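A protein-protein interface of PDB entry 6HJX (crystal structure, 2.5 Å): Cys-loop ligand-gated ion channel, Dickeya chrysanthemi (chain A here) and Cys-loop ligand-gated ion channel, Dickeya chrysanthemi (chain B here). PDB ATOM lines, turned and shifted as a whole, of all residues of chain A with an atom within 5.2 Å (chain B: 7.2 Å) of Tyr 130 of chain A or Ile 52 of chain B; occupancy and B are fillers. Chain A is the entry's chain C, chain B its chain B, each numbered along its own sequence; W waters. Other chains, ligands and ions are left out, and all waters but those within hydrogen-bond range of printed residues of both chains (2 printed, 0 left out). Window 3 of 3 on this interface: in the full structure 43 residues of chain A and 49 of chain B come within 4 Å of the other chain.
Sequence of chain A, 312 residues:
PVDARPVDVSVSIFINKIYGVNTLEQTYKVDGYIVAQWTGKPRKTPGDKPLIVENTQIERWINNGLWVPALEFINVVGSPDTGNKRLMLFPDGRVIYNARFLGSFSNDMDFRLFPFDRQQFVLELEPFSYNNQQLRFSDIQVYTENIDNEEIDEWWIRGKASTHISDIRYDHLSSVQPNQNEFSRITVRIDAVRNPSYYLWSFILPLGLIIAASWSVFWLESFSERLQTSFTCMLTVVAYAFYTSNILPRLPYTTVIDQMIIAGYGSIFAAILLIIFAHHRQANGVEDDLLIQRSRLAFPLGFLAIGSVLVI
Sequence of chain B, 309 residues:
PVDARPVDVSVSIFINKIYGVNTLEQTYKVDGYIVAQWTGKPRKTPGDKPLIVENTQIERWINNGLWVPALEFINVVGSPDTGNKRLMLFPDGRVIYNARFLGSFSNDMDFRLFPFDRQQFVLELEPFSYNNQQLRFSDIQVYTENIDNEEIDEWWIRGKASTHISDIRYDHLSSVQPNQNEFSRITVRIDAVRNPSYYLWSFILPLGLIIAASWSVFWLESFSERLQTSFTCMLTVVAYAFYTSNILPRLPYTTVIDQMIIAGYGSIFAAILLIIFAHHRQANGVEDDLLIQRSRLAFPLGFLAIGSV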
ATOM      1  N   TRP A  67      13.762   4.532  16.889  1.00  0.00           N
ATOM      2  CA  TRP A  67      14.538   3.981  17.989  1.00  0.00           C
ATOM      3  C   TRP A  67      13.906   2.679  18.464  1.00  0.00           C
ATOM      4  O   TRP A  67      12.774   2.678  18.962  1.00  0.00           O
ATOM      5  CB  TRP A  67      14.608   4.996  19.125  1.00  0.00           C
ATOM      6  CG  TRP A  67      15.451   4.570  20.278  1.00  0.00           C
ATOM      7  CD1 TRP A  67      16.799   4.378  20.274  1.00  0.00           C
ATOM      8  CD2 TRP A  67      15.008   4.300  21.616  1.00  0.00           C
ATOM      9  NE1 TRP A  67      17.226   4.001  21.524  1.00  0.00           N
ATOM     10  CE2 TRP A  67      16.146   3.945  22.366  1.00  0.00           C
ATOM     11  CE3 TRP A  67      13.762   4.320  22.250  1.00  0.00           C
ATOM     12  CZ2 TRP A  67      16.078   3.613  23.716  1.00  0.00           C
ATOM     13  CZ3 TRP A  67      13.696   3.990  23.596  1.00  0.00           C
ATOM     14  CH2 TRP A  67      14.847   3.641  24.312  1.00  0.00           C
ATOM     15  N   PRO A  69      15.364  -0.256  20.851  1.00  0.00           N
ATOM     16  CA  PRO A  69      16.553  -0.700  21.582  1.00  0.00           C
ATOM     17  C   PRO A  69      16.621  -2.209  21.740  1.00  0.00           C
ATOM     18  O   PRO A  69      15.609  -2.894  21.892  1.00  0.00           O
ATOM     19  CB  PRO A  69      16.396  -0.014  22.945  1.00  0.00           C
ATOM     20  CG  PRO A  69      14.920   0.092  23.128  1.00  0.00           C
ATOM     21  CD  PRO A  69      14.343   0.313  21.752  1.00  0.00           C
ATOM     22  N   ALA A  70      17.848  -2.721  21.716  1.00  0.00           N
ATOM     23  CA  ALA A  70      18.085  -4.140  21.927  1.00  0.00           C
ATOM     24  C   ALA A  70      18.002  -4.466  23.413  1.00  0.00           C
ATOM     25  O   ALA A  70      18.664  -3.827  24.237  1.00  0.00           O
ATOM     26  CB  ALA A  70      19.452  -4.542  21.377  1.00  0.00           C
ATOM     27  N   PRO A 127      18.656  -3.904  29.112  1.00  0.00           N
ATOM     28  CA  PRO A 127      19.033  -3.281  27.835  1.00  0.00           C
ATOM     29  C   PRO A 127      20.508  -3.507  27.548  1.00  0.00           C
ATOM     30  O   PRO A 127      21.351  -3.461  28.447  1.00  0.00           O
ATOM     31  CB  PRO A 127      18.716  -1.794  28.049  1.00  0.00           C
ATOM     32  CG  PRO A 127      17.813  -1.750  29.234  1.00  0.00           C
ATOM     33  CD  PRO A 127      18.218  -2.901  30.094  1.00  0.00           C
ATOM     34  N   PHE A 128      20.816  -3.761  26.277  1.00  0.00           N
ATOM     35  CA  PHE A 128      22.189  -4.070  25.897  1.00  0.00           C
ATOM     36  C   PHE A 128      23.076  -2.831  25.848  1.00  0.00           C
ATOM     37  O   PHE A 128      24.284  -2.937  26.088  1.00  0.00           O
ATOM     38  CB  PHE A 128      22.212  -4.771  24.537  1.00  0.00           C
ATOM     39  CG  PHE A 128      23.566  -5.288  24.147  1.00  0.00           C
ATOM     40  CD1 PHE A 128      24.097  -6.406  24.767  1.00  0.00           C
ATOM     41  CD2 PHE A 128      24.307  -4.659  23.159  1.00  0.00           C
ATOM     42  CE1 PHE A 128      25.346  -6.887  24.413  1.00  0.00           C
ATOM     43  CE2 PHE A 128      25.556  -5.132  22.799  1.00  0.00           C
ATOM     44  CZ  PHE A 128      26.077  -6.246  23.425  1.00  0.00           C
ATOM     45  N   SER A 129      22.509  -1.656  25.555  1.00  0.00           N
ATOM     46  CA  SER A 129      23.311  -0.473  25.267  1.00  0.00           C
ATOM     47  C   SER A 129      22.919   0.772  26.048  1.00  0.00           C
ATOM     48  O   SER A 129      23.699   1.731  26.060  1.00  0.00           O
ATOM     49  CB  SER A 129      23.239  -0.130  23.768  1.00  0.00           C
ATOM     50  OG  SER A 129      23.617  -1.234  22.967  1.00  0.00           O
ATOM     51  N   TYR A 130      21.760   0.797  26.697  1.00  0.00           N
ATOM     52  CA  TYR A 130      21.213   2.022  27.268  1.00  0.00           C
ATOM     53  C   TYR A 130      21.144   1.890  28.779  1.00  0.00           C
ATOM     54  O   TYR A 130      20.498   0.974  29.296  1.00  0.00           O
ATOM     55  CB  TYR A 130      19.840   2.316  26.664  1.00  0.00           C
ATOM     56  CG  TYR A 130      19.935   2.604  25.183  1.00  0.00           C
ATOM     57  CD1 TYR A 130      20.310   3.863  24.728  1.00  0.00           C
ATOM     58  CD2 TYR A 130      19.684   1.615  24.243  1.00  0.00           C
ATOM     59  CE1 TYR A 130      20.415   4.134  23.385  1.00  0.00           C
ATOM     60  CE2 TYR A 130      19.790   1.877  22.887  1.00  0.00           C
ATOM     61  CZ  TYR A 130      20.162   3.136  22.467  1.00  0.00           C
ATOM     62  OH  TYR A 130      20.259   3.407  21.122  1.00  0.00           O
ATOM     63  N   ASN A 131      21.826   2.795  29.482  1.00  0.00           N
ATOM     64  CA  ASN A 131      21.797   2.819  30.935  1.00  0.00           C
ATOM     65  C   ASN A 131      20.448   3.347  31.429  1.00  0.00           C
ATOM     66  O   ASN A 131      19.588   3.772  30.650  1.00  0.00           O
ATOM     67  CB  ASN A 131      22.951   3.669  31.477  1.00  0.00           C
ATOM     68  CG  ASN A 131      22.919   5.104  30.973  1.00  0.00           C
ATOM     69  OD1 ASN A 131      21.851   5.681  30.771  1.00  0.00           O
ATOM     70  ND2 ASN A 131      24.096   5.683  30.768  1.00  0.00           N
ATOM     71  N   ASN A 132      20.264   3.315  32.753  1.00  0.00           N
ATOM     72  CA  ASN A 132      18.985   3.715  33.329  1.00  0.00           C
ATOM     73  C   ASN A 132      18.760   5.225  33.297  1.00  0.00           C
ATOM     74  O   ASN A 132      17.700   5.678  33.747  1.00  0.00           O
ATOM     75  CB  ASN A 132      18.860   3.186  34.761  1.00  0.00           C
ATOM     76  CG  ASN A 132      19.942   3.702  35.686  1.00  0.00           C
ATOM     77  OD1 ASN A 132      20.617   4.689  35.396  1.00  0.00           O
ATOM     78  ND2 ASN A 132      20.100   3.037  36.827  1.00  0.00           N
ATOM     79  N   GLN A 134      18.872   6.565  30.248  1.00  0.00           N
ATOM     80  CA  GLN A 134      18.257   6.571  28.931  1.00  0.00           C
ATOM     81  C   GLN A 134      17.097   5.596  28.810  1.00  0.00           C
ATOM     82  O   GLN A 134      16.136   5.886  28.092  1.00  0.00           O
ATOM     83  CB  GLN A 134      19.305   6.227  27.862  1.00  0.00           C
ATOM     84  CG  GLN A 134      20.593   7.036  27.968  1.00  0.00           C
ATOM     85  CD  GLN A 134      21.671   6.543  27.019  1.00  0.00           C
ATOM     86  OE1 GLN A 134      21.857   7.094  25.932  1.00  0.00           O
ATOM     87  NE2 GLN A 134      22.386   5.498  27.426  1.00  0.00           N
ATOM     88  N   LEU A 135      17.158   4.460  29.502  1.00  0.00           N
ATOM     89  CA  LEU A 135      16.128   3.431  29.393  1.00  0.00           C
ATOM     90  C   LEU A 135      16.015   2.714  30.728  1.00  0.00           C
ATOM     91  O   LEU A 135      16.981   2.095  31.183  1.00  0.00           O
ATOM     92  CB  LEU A 135      16.471   2.442  28.279  1.00  0.00           C
ATOM     93  CG  LEU A 135      15.355   1.540  27.754  1.00  0.00           C
ATOM     94  CD1 LEU A 135      15.844   0.816  26.504  1.00  0.00           C
ATOM     95  CD2 LEU A 135      14.881   0.538  28.803  1.00  0.00           C
ATOM     96  N   PHE A 183      22.458   0.038  34.767  1.00  0.00           N
ATOM     97  CA  PHE A 183      21.462  -0.481  33.838  1.00  0.00           C
ATOM     98  C   PHE A 183      20.271  -1.049  34.599  1.00  0.00           C
ATOM     99  O   PHE A 183      20.426  -1.631  35.677  1.00  0.00           O
ATOM    100  CB  PHE A 183      22.083  -1.553  32.924  1.00  0.00           C
ATOM    101  CG  PHE A 183      22.974  -0.987  31.851  1.00  0.00           C
ATOM    102  CD1 PHE A 183      24.220  -0.471  32.164  1.00  0.00           C
ATOM    103  CD2 PHE A 183      22.560  -0.965  30.530  1.00  0.00           C
ATOM    104  CE1 PHE A 183      25.035   0.057  31.177  1.00  0.00           C
ATOM    105  CE2 PHE A 183      23.375  -0.445  29.541  1.00  0.00           C
ATOM    106  CZ  PHE A 183      24.612   0.070  29.868  1.00  0.00           C
ATOM    107  N   LYS B  49      26.900  14.147  21.367  1.00  0.00           N
ATOM    108  CA  LYS B  49      26.913  13.148  22.421  1.00  0.00           C
ATOM    109  C   LYS B  49      27.410  11.816  21.879  1.00  0.00           C
ATOM    110  O   LYS B  49      27.382  11.575  20.670  1.00  0.00           O
ATOM    111  CB  LYS B  49      25.510  12.974  23.015  1.00  0.00           C
ATOM    112  CG  LYS B  49      25.023  14.157  23.846  1.00  0.00           C
ATOM    113  CD  LYS B  49      23.727  13.837  24.589  1.00  0.00           C
ATOM    114  CE  LYS B  49      22.503  13.928  23.686  1.00  0.00           C
ATOM    115  NZ  LYS B  49      22.121  15.339  23.396  1.00  0.00           N
ATOM    116  N   PRO B  50      27.885  10.924  22.746  1.00  0.00           N
ATOM    117  CA  PRO B  50      28.217   9.571  22.287  1.00  0.00           C
ATOM    118  C   PRO B  50      27.028   8.944  21.577  1.00  0.00           C
ATOM    119  O   PRO B  50      25.885   9.067  22.019  1.00  0.00           O
ATOM    120  CB  PRO B  50      28.563   8.827  23.582  1.00  0.00           C
ATOM    121  CG  PRO B  50      28.946   9.894  24.549  1.00  0.00           C
ATOM    122  CD  PRO B  50      28.115  11.091  24.193  1.00  0.00           C
ATOM    123  N   LEU B  51      27.299   8.281  20.455  1.00  0.00           N
ATOM    124  CA  LEU B  51      26.262   7.650  19.650  1.00  0.00           C
ATOM    125  C   LEU B  51      26.327   6.137  19.808  1.00  0.00           C
ATOM    126  O   LEU B  51      27.413   5.548  19.812  1.00  0.00           O
ATOM    127  CB  LEU B  51      26.404   8.027  18.174  1.00  0.00           C
ATOM    128  CG  LEU B  51      25.335   7.471  17.231  1.00  0.00           C
ATOM    129  CD1 LEU B  51      23.958   7.985  17.608  1.00  0.00           C
ATOM    130  CD2 LEU B  51      25.661   7.830  15.785  1.00  0.00           C
ATOM    131  N   ILE B  52      25.157   5.516  19.938  1.00  0.00           N
ATOM    132  CA  ILE B  52      25.028   4.071  20.092  1.00  0.00           C
ATOM    133  C   ILE B  52      24.513   3.505  18.775  1.00  0.00           C
ATOM    134  O   ILE B  52      23.453   3.913  18.286  1.00  0.00           O
ATOM    135  CB  ILE B  52      24.099   3.714  21.264  1.00  0.00           C
ATOM    136  CG1 ILE B  52      24.851   3.888  22.587  1.00  0.00           C
ATOM    137  CG2 ILE B  52      23.555   2.290  21.133  1.00  0.00           C
ATOM    138  CD1 ILE B  52      23.962   3.867  23.821  1.00  0.00           C
ATOM    139  N   VAL B  53      25.267   2.568  18.203  1.00  0.00           N
ATOM    140  CA  VAL B  53      24.904   1.890  16.962  1.00  0.00           C
ATOM    141  C   VAL B  53      24.878   0.396  17.260  1.00  0.00           C
ATOM    142  O   VAL B  53      25.905  -0.184  17.632  1.00  0.00           O
ATOM    143  CB  VAL B  53      25.890   2.210  15.826  1.00  0.00           C
ATOM    144  CG1 VAL B  53      25.457   1.542  14.527  1.00  0.00           C
ATOM    145  CG2 VAL B  53      26.020   3.717  15.627  1.00  0.00           C
ATOM    146  N   GLU B  54      23.713  -0.224  17.096  1.00  0.00           N
ATOM    147  CA  GLU B  54      23.489  -1.596  17.525  1.00  0.00           C
ATOM    148  C   GLU B  54      23.306  -2.529  16.337  1.00  0.00           C
ATOM    149  O   GLU B  54      22.660  -2.175  15.345  1.00  0.00           O
ATOM    150  CB  GLU B  54      22.259  -1.688  18.433  1.00  0.00           C
ATOM    151  CG  GLU B  54      22.504  -1.252  19.870  1.00  0.00           C
ATOM    152  CD  GLU B  54      21.266  -1.385  20.735  1.00  0.00           C
ATOM    153  OE1 GLU B  54      20.145  -1.204  20.206  1.00  0.00           O
ATOM    154  OE2 GLU B  54      21.417  -1.678  21.939  1.00  0.00           O
ATOM    155  N   GLN B  57      22.746  -2.192  12.241  1.00  0.00           N
ATOM    156  CA  GLN B  57      23.078  -0.822  11.872  1.00  0.00           C
ATOM    157  C   GLN B  57      24.582  -0.607  11.792  1.00  0.00           C
ATOM    158  O   GLN B  57      25.029   0.353  11.155  1.00  0.00           O
ATOM    159  CB  GLN B  57      22.468   0.163  12.869  1.00  0.00           C
ATOM    160  CG  GLN B  57      20.957   0.212  12.839  1.00  0.00           C
ATOM    161  CD  GLN B  57      20.424   0.551  11.467  1.00  0.00           C
ATOM    162  OE1 GLN B  57      20.566   1.678  10.992  1.00  0.00           O
ATOM    163  NE2 GLN B  57      19.818  -0.430  10.811  1.00  0.00           N
ATOM    164  N   TRP B  61      27.174   1.605   8.878  1.00  0.00           N
ATOM    165  CA  TRP B  61      28.286   2.510   9.140  1.00  0.00           C
ATOM    166  C   TRP B  61      29.578   2.019   8.499  1.00  0.00           C
ATOM    167  O   TRP B  61      30.418   2.833   8.099  1.00  0.00           O
ATOM    168  CB  TRP B  61      28.478   2.685  10.647  1.00  0.00           C
ATOM    169  CG  TRP B  61      27.502   3.642  11.261  1.00  0.00           C
ATOM    170  CD1 TRP B  61      26.204   3.388  11.595  1.00  0.00           C
ATOM    171  CD2 TRP B  61      27.749   5.006  11.615  1.00  0.00           C
ATOM    172  NE1 TRP B  61      25.625   4.512  12.133  1.00  0.00           N
ATOM    173  CE2 TRP B  61      26.554   5.519  12.157  1.00  0.00           C
ATOM    174  CE3 TRP B  61      28.864   5.846  11.526  1.00  0.00           C
ATOM    175  CZ2 TRP B  61      26.443   6.833  12.608  1.00  0.00           C
ATOM    176  CZ3 TRP B  61      28.751   7.152  11.973  1.00  0.00           C
ATOM    177  CH2 TRP B  61      27.550   7.632  12.508  1.00  0.00           C
ATOM    178  N   ARG B  86      27.404  -3.911  19.615  1.00  0.00           N
ATOM    179  CA  ARG B  86      27.165  -2.486  19.785  1.00  0.00           C
ATOM    180  C   ARG B  86      28.435  -1.704  19.489  1.00  0.00           C
ATOM    181  O   ARG B  86      29.538  -2.140  19.829  1.00  0.00           O
ATOM    182  CB  ARG B  86      26.687  -2.185  21.213  1.00  0.00           C
ATOM    183  CG  ARG B  86      26.406  -0.717  21.506  1.00  0.00           C
ATOM    184  CD  ARG B  86      26.964  -0.312  22.862  1.00  0.00           C
ATOM    185  NE  ARG B  86      28.422  -0.380  22.886  1.00  0.00           N
ATOM    186  CZ  ARG B  86      29.175  -0.073  23.939  1.00  0.00           C
ATOM    187  NH1 ARG B  86      28.614   0.331  25.072  1.00  0.00           N
ATOM    188  NH2 ARG B  86      30.495  -0.168  23.860  1.00  0.00           N
ATOM    189  N   LEU B  87      28.265  -0.547  18.853  1.00  0.00           N
ATOM    190  CA  LEU B  87      29.319   0.445  18.712  1.00  0.00           C
ATOM    191  C   LEU B  87      28.893   1.688  19.480  1.00  0.00           C
ATOM    192  O   LEU B  87      27.748   2.138  19.347  1.00  0.00           O
ATOM    193  CB  LEU B  87      29.577   0.809  17.246  1.00  0.00           C
ATOM    194  CG  LEU B  87      30.248  -0.217  16.336  1.00  0.00           C
ATOM    195  CD1 LEU B  87      30.452   0.398  14.961  1.00  0.00           C
ATOM    196  CD2 LEU B  87      31.571  -0.693  16.911  1.00  0.00           C
ATOM    197  N   MET B  88      29.798   2.232  20.286  1.00  0.00           N
ATOM    198  CA  MET B  88      29.628   3.563  20.860  1.00  0.00           C
ATOM    199  C   MET B  88      30.640   4.474  20.177  1.00  0.00           C
ATOM    200  O   MET B  88      31.852   4.319  20.366  1.00  0.00           O
ATOM    201  CB  MET B  88      29.806   3.557  22.376  1.00  0.00           C
ATOM    202  CG  MET B  88      29.419   4.889  23.019  1.00  0.00           C
ATOM    203  SD  MET B  88      29.280   4.841  24.813  1.00  0.00           S
ATOM    204  CE  MET B  88      27.829   3.804  25.004  1.00  0.00           C
ATOM    205  N   LEU B  89      30.146   5.407  19.369  1.00  0.00           N
ATOM    206  CA  LEU B  89      30.993   6.282  18.570  1.00  0.00           C
ATOM    207  C   LEU B  89      31.029   7.663  19.207  1.00  0.00           C
ATOM    208  O   LEU B  89      29.994   8.330  19.311  1.00  0.00           O
ATOM    209  CB  LEU B  89      30.477   6.376  17.134  1.00  0.00           C
ATOM    210  CG  LEU B  89      30.298   5.045  16.408  1.00  0.00           C
ATOM    211  CD1 LEU B  89      29.687   5.273  15.035  1.00  0.00           C
ATOM    212  CD2 LEU B  89      31.615   4.312  16.298  1.00  0.00           C
HETATM  213  O   HOH W   1      19.389   1.367  19.598  1.00  0.00           O
HETATM  214  O   HOH W   2      20.067  -1.489  24.033  1.00  0.00           O
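Water W2 lies within hydrogen-bond range of the side-chain carboxylate (OE2) of Glu 54 of chain B, the backbone carbonyl oxygen (O) of Ala 70 of chain A, the backbone NH (N) of Ser 129 of chain A and the backbone NH (N) of Phe 128 of chain A.
Water W1 bridges the side-chain hydroxyl of Tyr 130 of chain A (2.7 Å) and the side-chain carboxylate of Glu 54 of chain B (2.7 Å).
Of the printed residues of chain B, Pro 69 of chain A touches Glu 54.
Of the printed residues of chain B, Ala 70 of chain A touches Glu 54.
Printed residues of chain B within 4 Å of Ser 129 of chain A: Ile 52, Glu 54 and Arg 86.
Tyr 130 of chain A touches just one residue of chain B: Ile 52 (3.5 Å).
Pro 50 of chain B touches none of the printed residues of chain A.
Of the printed residues of chain A, Ile 52 of chain B touches Ser 129 and Tyr 130.
The nearest residue of chain A that does not touch Ile 52 of chain B is Gln 134 of chain A (4.3 Å).
The nearest printed residue of chain B that does not touch Phe 128 of chain A is Glu 54 of chain B (4.1 Å).
N of Ala 70 of chain A sits at hydrogen-bond distance from OE1 of Glu 54 of chain B.
The side-chain hydroxyl of Ser 129 of chain A is in hydrogen-bond range of the side-chain carboxylate of Glu 54 of chain B, 2.5 Å away.
Printed residues of chain A that touch a printed residue of chain B: Pro 69, Ala 70, Phe 128, Ser 129 and Tyr 130.
Hydrophobic or aromatic side chains of chain A within 4 Å of the printed part of chain B: Ala 70, Phe 128 and Tyr 130.
Among the printed residues, no Asp or Glu carboxylate lies within 4 Å of a Lys or Arg side-chain nitrogen of the other chain.
Glu 54 of chain B touches Pro 69 of chain A.
Arg 86 of chain B touches Phe 128 of chain A (CB to CE2, 3.5 Å).
Ile 52 of chain B touches Ser 129 of chain A (CD1 to O, 3.1 Å).
Arg 86 of chain B touches Ser 129 of chain A (CG to OG, 3.2 Å).
OH of Tyr 130 of chain A touches CG2 of Ile 52 of chain B, at 3.5 Å.
The indole nitrogen of Trp 67 of chain A is in hydrogen-bond range of the side-chain hydroxyl of Tyr 130 of chain A.
O of Ala 70 of chain A sits at hydrogen-bond distance from N of Phe 128 of chain A.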
